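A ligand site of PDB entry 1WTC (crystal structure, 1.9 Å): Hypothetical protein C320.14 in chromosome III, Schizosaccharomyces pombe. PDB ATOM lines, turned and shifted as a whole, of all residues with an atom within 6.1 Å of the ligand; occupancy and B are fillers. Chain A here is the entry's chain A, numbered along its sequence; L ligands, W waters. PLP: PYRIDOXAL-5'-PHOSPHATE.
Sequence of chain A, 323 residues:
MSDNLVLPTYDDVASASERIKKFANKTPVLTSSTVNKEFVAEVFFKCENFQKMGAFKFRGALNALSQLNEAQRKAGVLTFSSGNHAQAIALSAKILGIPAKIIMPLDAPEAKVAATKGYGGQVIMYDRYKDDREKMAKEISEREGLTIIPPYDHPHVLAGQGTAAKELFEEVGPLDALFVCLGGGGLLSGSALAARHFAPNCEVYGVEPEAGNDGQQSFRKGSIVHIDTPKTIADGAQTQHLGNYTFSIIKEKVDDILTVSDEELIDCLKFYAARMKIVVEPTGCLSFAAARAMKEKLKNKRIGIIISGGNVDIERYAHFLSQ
Water W1 lies within hydrogen-bond range of an oxygen (O2P) of the ligand (2.6 Å), the backbone carbonyl oxygen of Cys 181 (2.7 Å), the backbone NH of Leu 188 (2.7 Å) and the backbone NH of Leu 187 (3.5 Å). Water W2 lies within hydrogen-bond range of an oxygen (O3P) of the ligand, the backbone carbonyl oxygen (O) of Pro 151 and the side-chain amide nitrogen (NE2) of Gln 161. Water W3 bridges N of Asn 84 (2.9 Å) and O3 of the ligand (2.9 Å). Water W4 lies within hydrogen-bond range of O of Gly 236 (2.8 Å) and O1P of the ligand (3.0 Å).
The backbone carbonyl oxygen (O) of Thr 283 sits at hydrogen-bond distance from the side-chain sulfur (SG) of Cys 181 (3.7 Å). O of Gly 184 sits at hydrogen-bond distance from OG1 of Thr 246 (3.0 Å). OE2 of Glu 281 sits at hydrogen-bond distance from ND2 of Asn 84, 3.0 Å away. OG of Ser 308 is in hydrogen-bond range of SG of Cys 181 (3.5 Å). The backbone NH of Gly 236 is in hydrogen-bond range of the side-chain hydroxyl of Thr 283, 2.8 Å away. The backbone carbonyl oxygen of Gly 183 sits at hydrogen-bond distance from the side-chain hydroxyl of Thr 239 (2.6 Å). The backbone carbonyl oxygen (O) of Ser 308 sits at hydrogen-bond distance from the backbone NH (N) of Phe 56 (3.0 Å). O of Gly 309 sits at hydrogen-bond distance from N of Glu 281.
An oxygen (O3P) of the ligand sits at hydrogen-bond distance from the backbone NH of Gly 186 (2.8 Å). An oxygen (O3P) of the ligand lies within hydrogen-bond range of the backbone NH (N) of Leu 187 (2.8 Å). N of Gly 183 sits at hydrogen-bond distance from O2P of the ligand (2.7 Å). OG of Ser 308 sits at hydrogen-bond distance from N1 of the ligand (2.7 Å). O1P of the ligand sits at hydrogen-bond distance from N of Gly 184 (2.7 Å). NZ of Lys 57 is bonded to C4A of the ligand. The backbone NH (N) of Gly 185 sits at hydrogen-bond distance from an oxygen (O2P) of the ligand (2.7 Å). An oxygen (O3) of the ligand lies within hydrogen-bond range of the side-chain amide nitrogen of Asn 84 (2.7 Å).
Phe 56 touches the ligand. Tyr 152 touches the ligand. CB of Cys 181 touches C6 of the ligand, at 3.9 Å. C of Leu 182 touches O2P of the ligand, at 3.8 Å. Gly 236 touches the ligand. Glu 281 touches the ligand (CD to C2A, 3.4 Å). CG2 of Thr 283 touches N1 of the ligand, 3.4 Å away. Gly 309 touches the ligand (N to C2A, 3.8 Å). Hydrophobic or aromatic side chains within 4 Å of the ligand: Phe 56, Tyr 152 and Leu 187.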
ATOM      1  N   ALA A  55      -7.247 -32.327  -9.398  1.00  0.00           N
ATOM      2  CA  ALA A  55      -6.664 -31.835  -8.151  1.00  0.00           C
ATOM      3  C   ALA A  55      -6.560 -32.935  -7.102  1.00  0.00           C
ATOM      4  O   ALA A  55      -7.307 -33.916  -7.135  1.00  0.00           O
ATOM      5  CB  ALA A  55      -7.485 -30.664  -7.598  1.00  0.00           C
ATOM      6  N   PHE A  56      -5.619 -32.786  -6.175  1.00  0.00           N
ATOM      7  CA  PHE A  56      -5.407 -33.781  -5.132  1.00  0.00           C
ATOM      8  C   PHE A  56      -6.679 -34.140  -4.362  1.00  0.00           C
ATOM      9  O   PHE A  56      -6.842 -35.271  -3.902  1.00  0.00           O
ATOM     10  CB  PHE A  56      -4.343 -33.272  -4.138  1.00  0.00           C
ATOM     11  CG  PHE A  56      -4.851 -32.229  -3.169  1.00  0.00           C
ATOM     12  CD1 PHE A  56      -5.420 -32.607  -1.956  1.00  0.00           C
ATOM     13  CD2 PHE A  56      -4.744 -30.868  -3.457  1.00  0.00           C
ATOM     14  CE1 PHE A  56      -5.866 -31.654  -1.046  1.00  0.00           C
ATOM     15  CE2 PHE A  56      -5.186 -29.906  -2.562  1.00  0.00           C
ATOM     16  CZ  PHE A  56      -5.751 -30.293  -1.346  1.00  0.00           C
ATOM     17  N   LYS A  57      -7.580 -33.161  -4.234  1.00  0.00           N
ATOM     18  CA  LYS A  57      -8.836 -33.313  -3.494  1.00  0.00           C
ATOM     19  C   LYS A  57      -9.593 -34.605  -3.743  1.00  0.00           C
ATOM     20  O   LYS A  57     -10.337 -35.059  -2.874  1.00  0.00           O
ATOM     21  CB  LYS A  57      -9.759 -32.133  -3.795  1.00  0.00           C
ATOM     22  CG  LYS A  57      -9.255 -30.767  -3.353  1.00  0.00           C
ATOM     23  CD  LYS A  57      -9.640 -30.462  -1.926  1.00  0.00           C
ATOM     24  CE  LYS A  57      -9.944 -28.971  -1.746  1.00  0.00           C
ATOM     25  NZ  LYS A  57      -8.781 -28.313  -2.345  1.00  0.00           N
ATOM     26  N   GLY A  83     -14.639 -24.337  -4.315  1.00  0.00           N
ATOM     27  CA  GLY A  83     -13.354 -24.862  -4.736  1.00  0.00           C
ATOM     28  C   GLY A  83     -13.384 -26.268  -5.301  1.00  0.00           C
ATOM     29  O   GLY A  83     -14.453 -26.830  -5.543  1.00  0.00           O
ATOM     30  N   ASN A  84     -12.209 -26.843  -5.497  1.00  0.00           N
ATOM     31  CA  ASN A  84     -12.077 -28.197  -6.052  1.00  0.00           C
ATOM     32  C   ASN A  84     -12.775 -29.302  -5.266  1.00  0.00           C
ATOM     33  O   ASN A  84     -13.022 -30.370  -5.822  1.00  0.00           O
ATOM     34  CB  ASN A  84     -10.595 -28.565  -6.192  1.00  0.00           C
ATOM     35  CG  ASN A  84      -9.949 -27.912  -7.386  1.00  0.00           C
ATOM     36  OD1 ASN A  84     -10.486 -27.952  -8.482  1.00  0.00           O
ATOM     37  ND2 ASN A  84      -8.780 -27.321  -7.176  1.00  0.00           N
ATOM     38  N   HIS A  85     -13.084 -29.065  -4.005  1.00  0.00           N
ATOM     39  CA  HIS A  85     -13.730 -30.087  -3.183  1.00  0.00           C
ATOM     40  C   HIS A  85     -15.073 -30.482  -3.787  1.00  0.00           C
ATOM     41  O   HIS A  85     -15.457 -31.656  -3.781  1.00  0.00           O
ATOM     42  CB  HIS A  85     -13.920 -29.573  -1.739  1.00  0.00           C
ATOM     43  CG  HIS A  85     -14.482 -30.598  -0.795  1.00  0.00           C
ATOM     44  ND1 HIS A  85     -13.851 -31.801  -0.540  1.00  0.00           N
ATOM     45  CD2 HIS A  85     -15.588 -30.585  -0.015  1.00  0.00           C
ATOM     46  CE1 HIS A  85     -14.553 -32.473   0.360  1.00  0.00           C
ATOM     47  NE2 HIS A  85     -15.603 -31.760   0.697  1.00  0.00           N
ATOM     48  N   PRO A 151     -14.347 -29.847   3.440  1.00  0.00           N
ATOM     49  CA  PRO A 151     -13.324 -29.748   2.403  1.00  0.00           C
ATOM     50  C   PRO A 151     -11.909 -30.012   2.901  1.00  0.00           C
ATOM     51  O   PRO A 151     -10.997 -30.297   2.116  1.00  0.00           O
ATOM     52  CB  PRO A 151     -13.516 -28.337   1.841  1.00  0.00           C
ATOM     53  CG  PRO A 151     -14.176 -27.577   2.961  1.00  0.00           C
ATOM     54  CD  PRO A 151     -15.133 -28.591   3.536  1.00  0.00           C
ATOM     55  N   TYR A 152     -11.706 -29.931   4.220  1.00  0.00           N
ATOM     56  CA  TYR A 152     -10.395 -30.191   4.804  1.00  0.00           C
ATOM     57  C   TYR A 152     -10.391 -30.653   6.263  1.00  0.00           C
ATOM     58  O   TYR A 152      -9.605 -31.517   6.628  1.00  0.00           O
ATOM     59  CB  TYR A 152      -9.488 -28.956   4.650  1.00  0.00           C
ATOM     60  CG  TYR A 152     -10.059 -27.668   5.205  1.00  0.00           C
ATOM     61  CD1 TYR A 152     -10.021 -27.385   6.568  1.00  0.00           C
ATOM     62  CD2 TYR A 152     -10.652 -26.722   4.360  1.00  0.00           C
ATOM     63  CE1 TYR A 152     -10.537 -26.187   7.077  1.00  0.00           C
ATOM     64  CE2 TYR A 152     -11.170 -25.527   4.860  1.00  0.00           C
ATOM     65  CZ  TYR A 152     -11.115 -25.272   6.217  1.00  0.00           C
ATOM     66  OH  TYR A 152     -11.615 -24.087   6.695  1.00  0.00           O
ATOM     67  N   GLN A 161      -5.732 -36.940   1.461  1.00  0.00           N
ATOM     68  CA  GLN A 161      -4.836 -35.977   0.819  1.00  0.00           C
ATOM     69  C   GLN A 161      -3.390 -36.419   1.046  1.00  0.00           C
ATOM     70  O   GLN A 161      -2.546 -36.327   0.159  1.00  0.00           O
ATOM     71  CB  GLN A 161      -5.036 -34.572   1.414  1.00  0.00           C
ATOM     72  CG  GLN A 161      -6.460 -34.204   1.768  1.00  0.00           C
ATOM     73  CD  GLN A 161      -7.400 -34.202   0.574  1.00  0.00           C
ATOM     74  OE1 GLN A 161      -7.284 -35.024  -0.329  1.00  0.00           O
ATOM     75  NE2 GLN A 161      -8.365 -33.289   0.577  1.00  0.00           N
ATOM     76  N   CYS A 181       1.076 -26.653  -0.389  1.00  0.00           N
ATOM     77  CA  CYS A 181       0.126 -25.555  -0.408  1.00  0.00           C
ATOM     78  C   CYS A 181      -0.717 -25.586   0.846  1.00  0.00           C
ATOM     79  O   CYS A 181      -1.074 -26.662   1.331  1.00  0.00           O
ATOM     80  CB  CYS A 181      -0.757 -25.684  -1.646  1.00  0.00           C
ATOM     81  SG  CYS A 181       0.165 -26.112  -3.141  1.00  0.00           S
ATOM     82  N   LEU A 182      -1.034 -24.423   1.398  1.00  0.00           N
ATOM     83  CA  LEU A 182      -1.826 -24.381   2.605  1.00  0.00           C
ATOM     84  C   LEU A 182      -3.062 -23.508   2.510  1.00  0.00           C
ATOM     85  O   LEU A 182      -2.977 -22.289   2.296  1.00  0.00           O
ATOM     86  CB  LEU A 182      -0.994 -23.910   3.793  1.00  0.00           C
ATOM     87  CG  LEU A 182      -1.797 -23.709   5.079  1.00  0.00           C
ATOM     88  CD1 LEU A 182      -2.429 -25.038   5.495  1.00  0.00           C
ATOM     89  CD2 LEU A 182      -0.904 -23.190   6.194  1.00  0.00           C
ATOM     90  N   GLY A 183      -4.218 -24.141   2.678  1.00  0.00           N
ATOM     91  CA  GLY A 183      -5.484 -23.425   2.653  1.00  0.00           C
ATOM     92  C   GLY A 183      -6.155 -23.689   3.990  1.00  0.00           C
ATOM     93  O   GLY A 183      -6.032 -22.901   4.927  1.00  0.00           O
ATOM     94  N   GLY A 184      -6.844 -24.817   4.071  1.00  0.00           N
ATOM     95  CA  GLY A 184      -7.525 -25.213   5.293  1.00  0.00           C
ATOM     96  C   GLY A 184      -6.632 -26.144   6.099  1.00  0.00           C
ATOM     97  O   GLY A 184      -6.856 -26.342   7.294  1.00  0.00           O
ATOM     98  N   GLY A 185      -5.634 -26.725   5.448  1.00  0.00           N
ATOM     99  CA  GLY A 185      -4.715 -27.608   6.145  1.00  0.00           C
ATOM    100  C   GLY A 185      -4.843 -29.097   5.877  1.00  0.00           C
ATOM    101  O   GLY A 185      -4.083 -29.890   6.429  1.00  0.00           O
ATOM    102  N   GLY A 186      -5.804 -29.482   5.045  1.00  0.00           N
ATOM    103  CA  GLY A 186      -5.985 -30.900   4.744  1.00  0.00           C
ATOM    104  C   GLY A 186      -4.774 -31.497   4.061  1.00  0.00           C
ATOM    105  O   GLY A 186      -4.245 -32.527   4.496  1.00  0.00           O
ATOM    106  N   LEU A 187      -4.328 -30.857   2.981  1.00  0.00           N
ATOM    107  CA  LEU A 187      -3.166 -31.341   2.250  1.00  0.00           C
ATOM    108  C   LEU A 187      -1.917 -31.253   3.130  1.00  0.00           C
ATOM    109  O   LEU A 187      -1.077 -32.147   3.126  1.00  0.00           O
ATOM    110  CB  LEU A 187      -2.954 -30.520   0.978  1.00  0.00           C
ATOM    111  CG  LEU A 187      -1.762 -30.917   0.114  1.00  0.00           C
ATOM    112  CD1 LEU A 187      -2.002 -32.294  -0.501  1.00  0.00           C
ATOM    113  CD2 LEU A 187      -1.536 -29.882  -0.986  1.00  0.00           C
ATOM    114  N   LEU A 188      -1.813 -30.157   3.880  1.00  0.00           N
ATOM    115  CA  LEU A 188      -0.654 -29.930   4.744  1.00  0.00           C
ATOM    116  C   LEU A 188      -0.506 -30.980   5.841  1.00  0.00           C
ATOM    117  O   LEU A 188       0.569 -31.539   6.028  1.00  0.00           O
ATOM    118  CB  LEU A 188      -0.735 -28.547   5.384  1.00  0.00           C
ATOM    119  CG  LEU A 188       0.489 -28.160   6.223  1.00  0.00           C
ATOM    120  CD1 LEU A 188       1.740 -28.401   5.412  1.00  0.00           C
ATOM    121  CD2 LEU A 188       0.406 -26.699   6.655  1.00  0.00           C
ATOM    122  N   GLY A 236      -7.839 -20.993  -4.395  1.00  0.00           N
ATOM    123  CA  GLY A 236      -8.018 -22.229  -3.637  1.00  0.00           C
ATOM    124  C   GLY A 236      -7.401 -22.170  -2.241  1.00  0.00           C
ATOM    125  O   GLY A 236      -7.432 -23.161  -1.512  1.00  0.00           O
ATOM    126  N   ALA A 237      -6.843 -21.015  -1.891  1.00  0.00           N
ATOM    127  CA  ALA A 237      -6.225 -20.835  -0.579  1.00  0.00           C
ATOM    128  C   ALA A 237      -6.721 -19.571   0.119  1.00  0.00           C
ATOM    129  O   ALA A 237      -5.982 -18.927   0.870  1.00  0.00           O
ATOM    130  CB  ALA A 237      -4.698 -20.786  -0.740  1.00  0.00           C
ATOM    131  N   THR A 239      -9.125 -19.518   2.327  1.00  0.00           N
ATOM    132  CA  THR A 239      -9.839 -19.915   3.547  1.00  0.00           C
ATOM    133  C   THR A 239      -9.587 -18.874   4.639  1.00  0.00           C
ATOM    134  O   THR A 239      -8.573 -18.177   4.632  1.00  0.00           O
ATOM    135  CB  THR A 239      -9.407 -21.315   4.052  1.00  0.00           C
ATOM    136  OG1 THR A 239      -7.976 -21.444   3.940  1.00  0.00           O
ATOM    137  CG2 THR A 239     -10.076 -22.409   3.243  1.00  0.00           C
ATOM    138  N   THR A 246      -6.656 -30.425  11.245  1.00  0.00           N
ATOM    139  CA  THR A 246      -5.520 -30.017  10.435  1.00  0.00           C
ATOM    140  C   THR A 246      -4.439 -29.286  11.243  1.00  0.00           C
ATOM    141  O   THR A 246      -3.266 -29.659  11.195  1.00  0.00           O
ATOM    142  CB  THR A 246      -5.968 -29.126   9.243  1.00  0.00           C
ATOM    143  OG1 THR A 246      -6.752 -28.033   9.738  1.00  0.00           O
ATOM    144  CG2 THR A 246      -6.814 -29.943   8.271  1.00  0.00           C
ATOM    145  N   GLU A 281      -2.973 -24.487 -11.737  1.00  0.00           N
ATOM    146  CA  GLU A 281      -3.755 -23.337 -11.283  1.00  0.00           C
ATOM    147  C   GLU A 281      -2.936 -22.531 -10.270  1.00  0.00           C
ATOM    148  O   GLU A 281      -2.077 -23.065  -9.579  1.00  0.00           O
ATOM    149  CB  GLU A 281      -5.096 -23.784 -10.673  1.00  0.00           C
ATOM    150  CG  GLU A 281      -5.015 -24.783  -9.535  1.00  0.00           C
ATOM    151  CD  GLU A 281      -6.395 -25.143  -8.999  1.00  0.00           C
ATOM    152  OE1 GLU A 281      -7.055 -24.285  -8.366  1.00  0.00           O
ATOM    153  OE2 GLU A 281      -6.831 -26.287  -9.229  1.00  0.00           O
ATOM    154  N   THR A 283      -3.189 -21.379  -7.216  1.00  0.00           N
ATOM    155  CA  THR A 283      -3.006 -21.915  -5.879  1.00  0.00           C
ATOM    156  C   THR A 283      -1.989 -23.052  -5.894  1.00  0.00           C
ATOM    157  O   THR A 283      -1.255 -23.252  -4.911  1.00  0.00           O
ATOM    158  CB  THR A 283      -4.326 -22.442  -5.311  1.00  0.00           C
ATOM    159  OG1 THR A 283      -5.371 -21.503  -5.601  1.00  0.00           O
ATOM    160  CG2 THR A 283      -4.229 -22.589  -3.784  1.00  0.00           C
ATOM    161  N   GLY A 284      -1.934 -23.786  -7.007  1.00  0.00           N
ATOM    162  CA  GLY A 284      -0.991 -24.886  -7.115  1.00  0.00           C
ATOM    163  C   GLY A 284       0.459 -24.458  -7.268  1.00  0.00           C
ATOM    164  O   GLY A 284       1.351 -25.291  -7.325  1.00  0.00           O
ATOM    165  N   LEU A 286       1.908 -22.123  -5.098  1.00  0.00           N
ATOM    166  CA  LEU A 286       2.418 -21.671  -3.811  1.00  0.00           C
ATOM    167  C   LEU A 286       3.709 -22.389  -3.402  1.00  0.00           C
ATOM    168  O   LEU A 286       4.739 -21.743  -3.202  1.00  0.00           O
ATOM    169  CB  LEU A 286       1.340 -21.834  -2.730  1.00  0.00           C
ATOM    170  CG  LEU A 286       0.156 -20.847  -2.799  1.00  0.00           C
ATOM    171  CD1 LEU A 286      -1.008 -21.344  -1.953  1.00  0.00           C
ATOM    172  CD2 LEU A 286       0.611 -19.470  -2.329  1.00  0.00           C
ATOM    173  N   SER A 308      -0.682 -29.000  -6.217  1.00  0.00           N
ATOM    174  CA  SER A 308      -2.036 -29.345  -5.790  1.00  0.00           C
ATOM    175  C   SER A 308      -3.123 -29.487  -6.860  1.00  0.00           C
ATOM    176  O   SER A 308      -4.055 -30.274  -6.679  1.00  0.00           O
ATOM    177  CB  SER A 308      -2.495 -28.338  -4.734  1.00  0.00           C
ATOM    178  OG  SER A 308      -2.491 -27.017  -5.244  1.00  0.00           O
ATOM    179  N   GLY A 309      -3.016 -28.762  -7.969  1.00  0.00           N
ATOM    180  CA  GLY A 309      -4.054 -28.892  -8.978  1.00  0.00           C
ATOM    181  C   GLY A 309      -3.880 -28.069 -10.232  1.00  0.00           C
ATOM    182  O   GLY A 309      -3.036 -27.171 -10.280  1.00  0.00           O
ATOM    183  N   GLY A 310      -4.672 -28.384 -11.255  1.00  0.00           N
ATOM    184  CA  GLY A 310      -4.584 -27.649 -12.514  1.00  0.00           C
ATOM    185  C   GLY A 310      -5.917 -27.145 -13.014  1.00  0.00           C
ATOM    186  O   GLY A 310      -6.099 -26.948 -14.215  1.00  0.00           O
HETATM  187  N1  PLP L   1      -4.555 -25.974  -3.790  1.00  0.00           N
HETATM  188  C2  PLP L   1      -5.632 -26.441  -4.515  1.00  0.00           C
HETATM  189  C2A PLP L   1      -5.506 -26.525  -6.068  1.00  0.00           C
HETATM  190  C3  PLP L   1      -6.801 -26.836  -3.864  1.00  0.00           C
HETATM  191  O3  PLP L   1      -7.904 -27.306  -4.604  1.00  0.00           O
HETATM  192  C4  PLP L   1      -6.877 -26.745  -2.486  1.00  0.00           C
HETATM  193  C4A PLP L   1      -8.190 -27.207  -1.802  1.00  0.00           C
HETATM  194  C5  PLP L   1      -5.749 -26.270  -1.765  1.00  0.00           C
HETATM  195  C6  PLP L   1      -4.622 -25.896  -2.432  1.00  0.00           C
HETATM  196  C5A PLP L   1      -5.721 -26.119  -0.215  1.00  0.00           C
HETATM  197  O4P PLP L   1      -5.701 -27.396   0.480  1.00  0.00           O
HETATM  198  P   PLP L   1      -6.257 -27.451   1.992  1.00  0.00           P
HETATM  199  O1P PLP L   1      -7.461 -26.604   2.178  1.00  0.00           O
HETATM  200  O2P PLP L   1      -5.105 -26.702   2.767  1.00  0.00           O
HETATM  201  O3P PLP L   1      -6.272 -28.889   2.361  1.00  0.00           O
HETATM  202  O   HOH W   1      -2.760 -27.745   3.105  1.00  0.00           O
HETATM  203  O   HOH W   2      -8.267 -30.795   2.217  1.00  0.00           O
HETATM  204  O   HOH W   3      -9.992 -25.224  -4.648  1.00  0.00           O
HETATM  205  O   HOH W   4      -8.929 -24.605   0.418  1.00  0.00           O
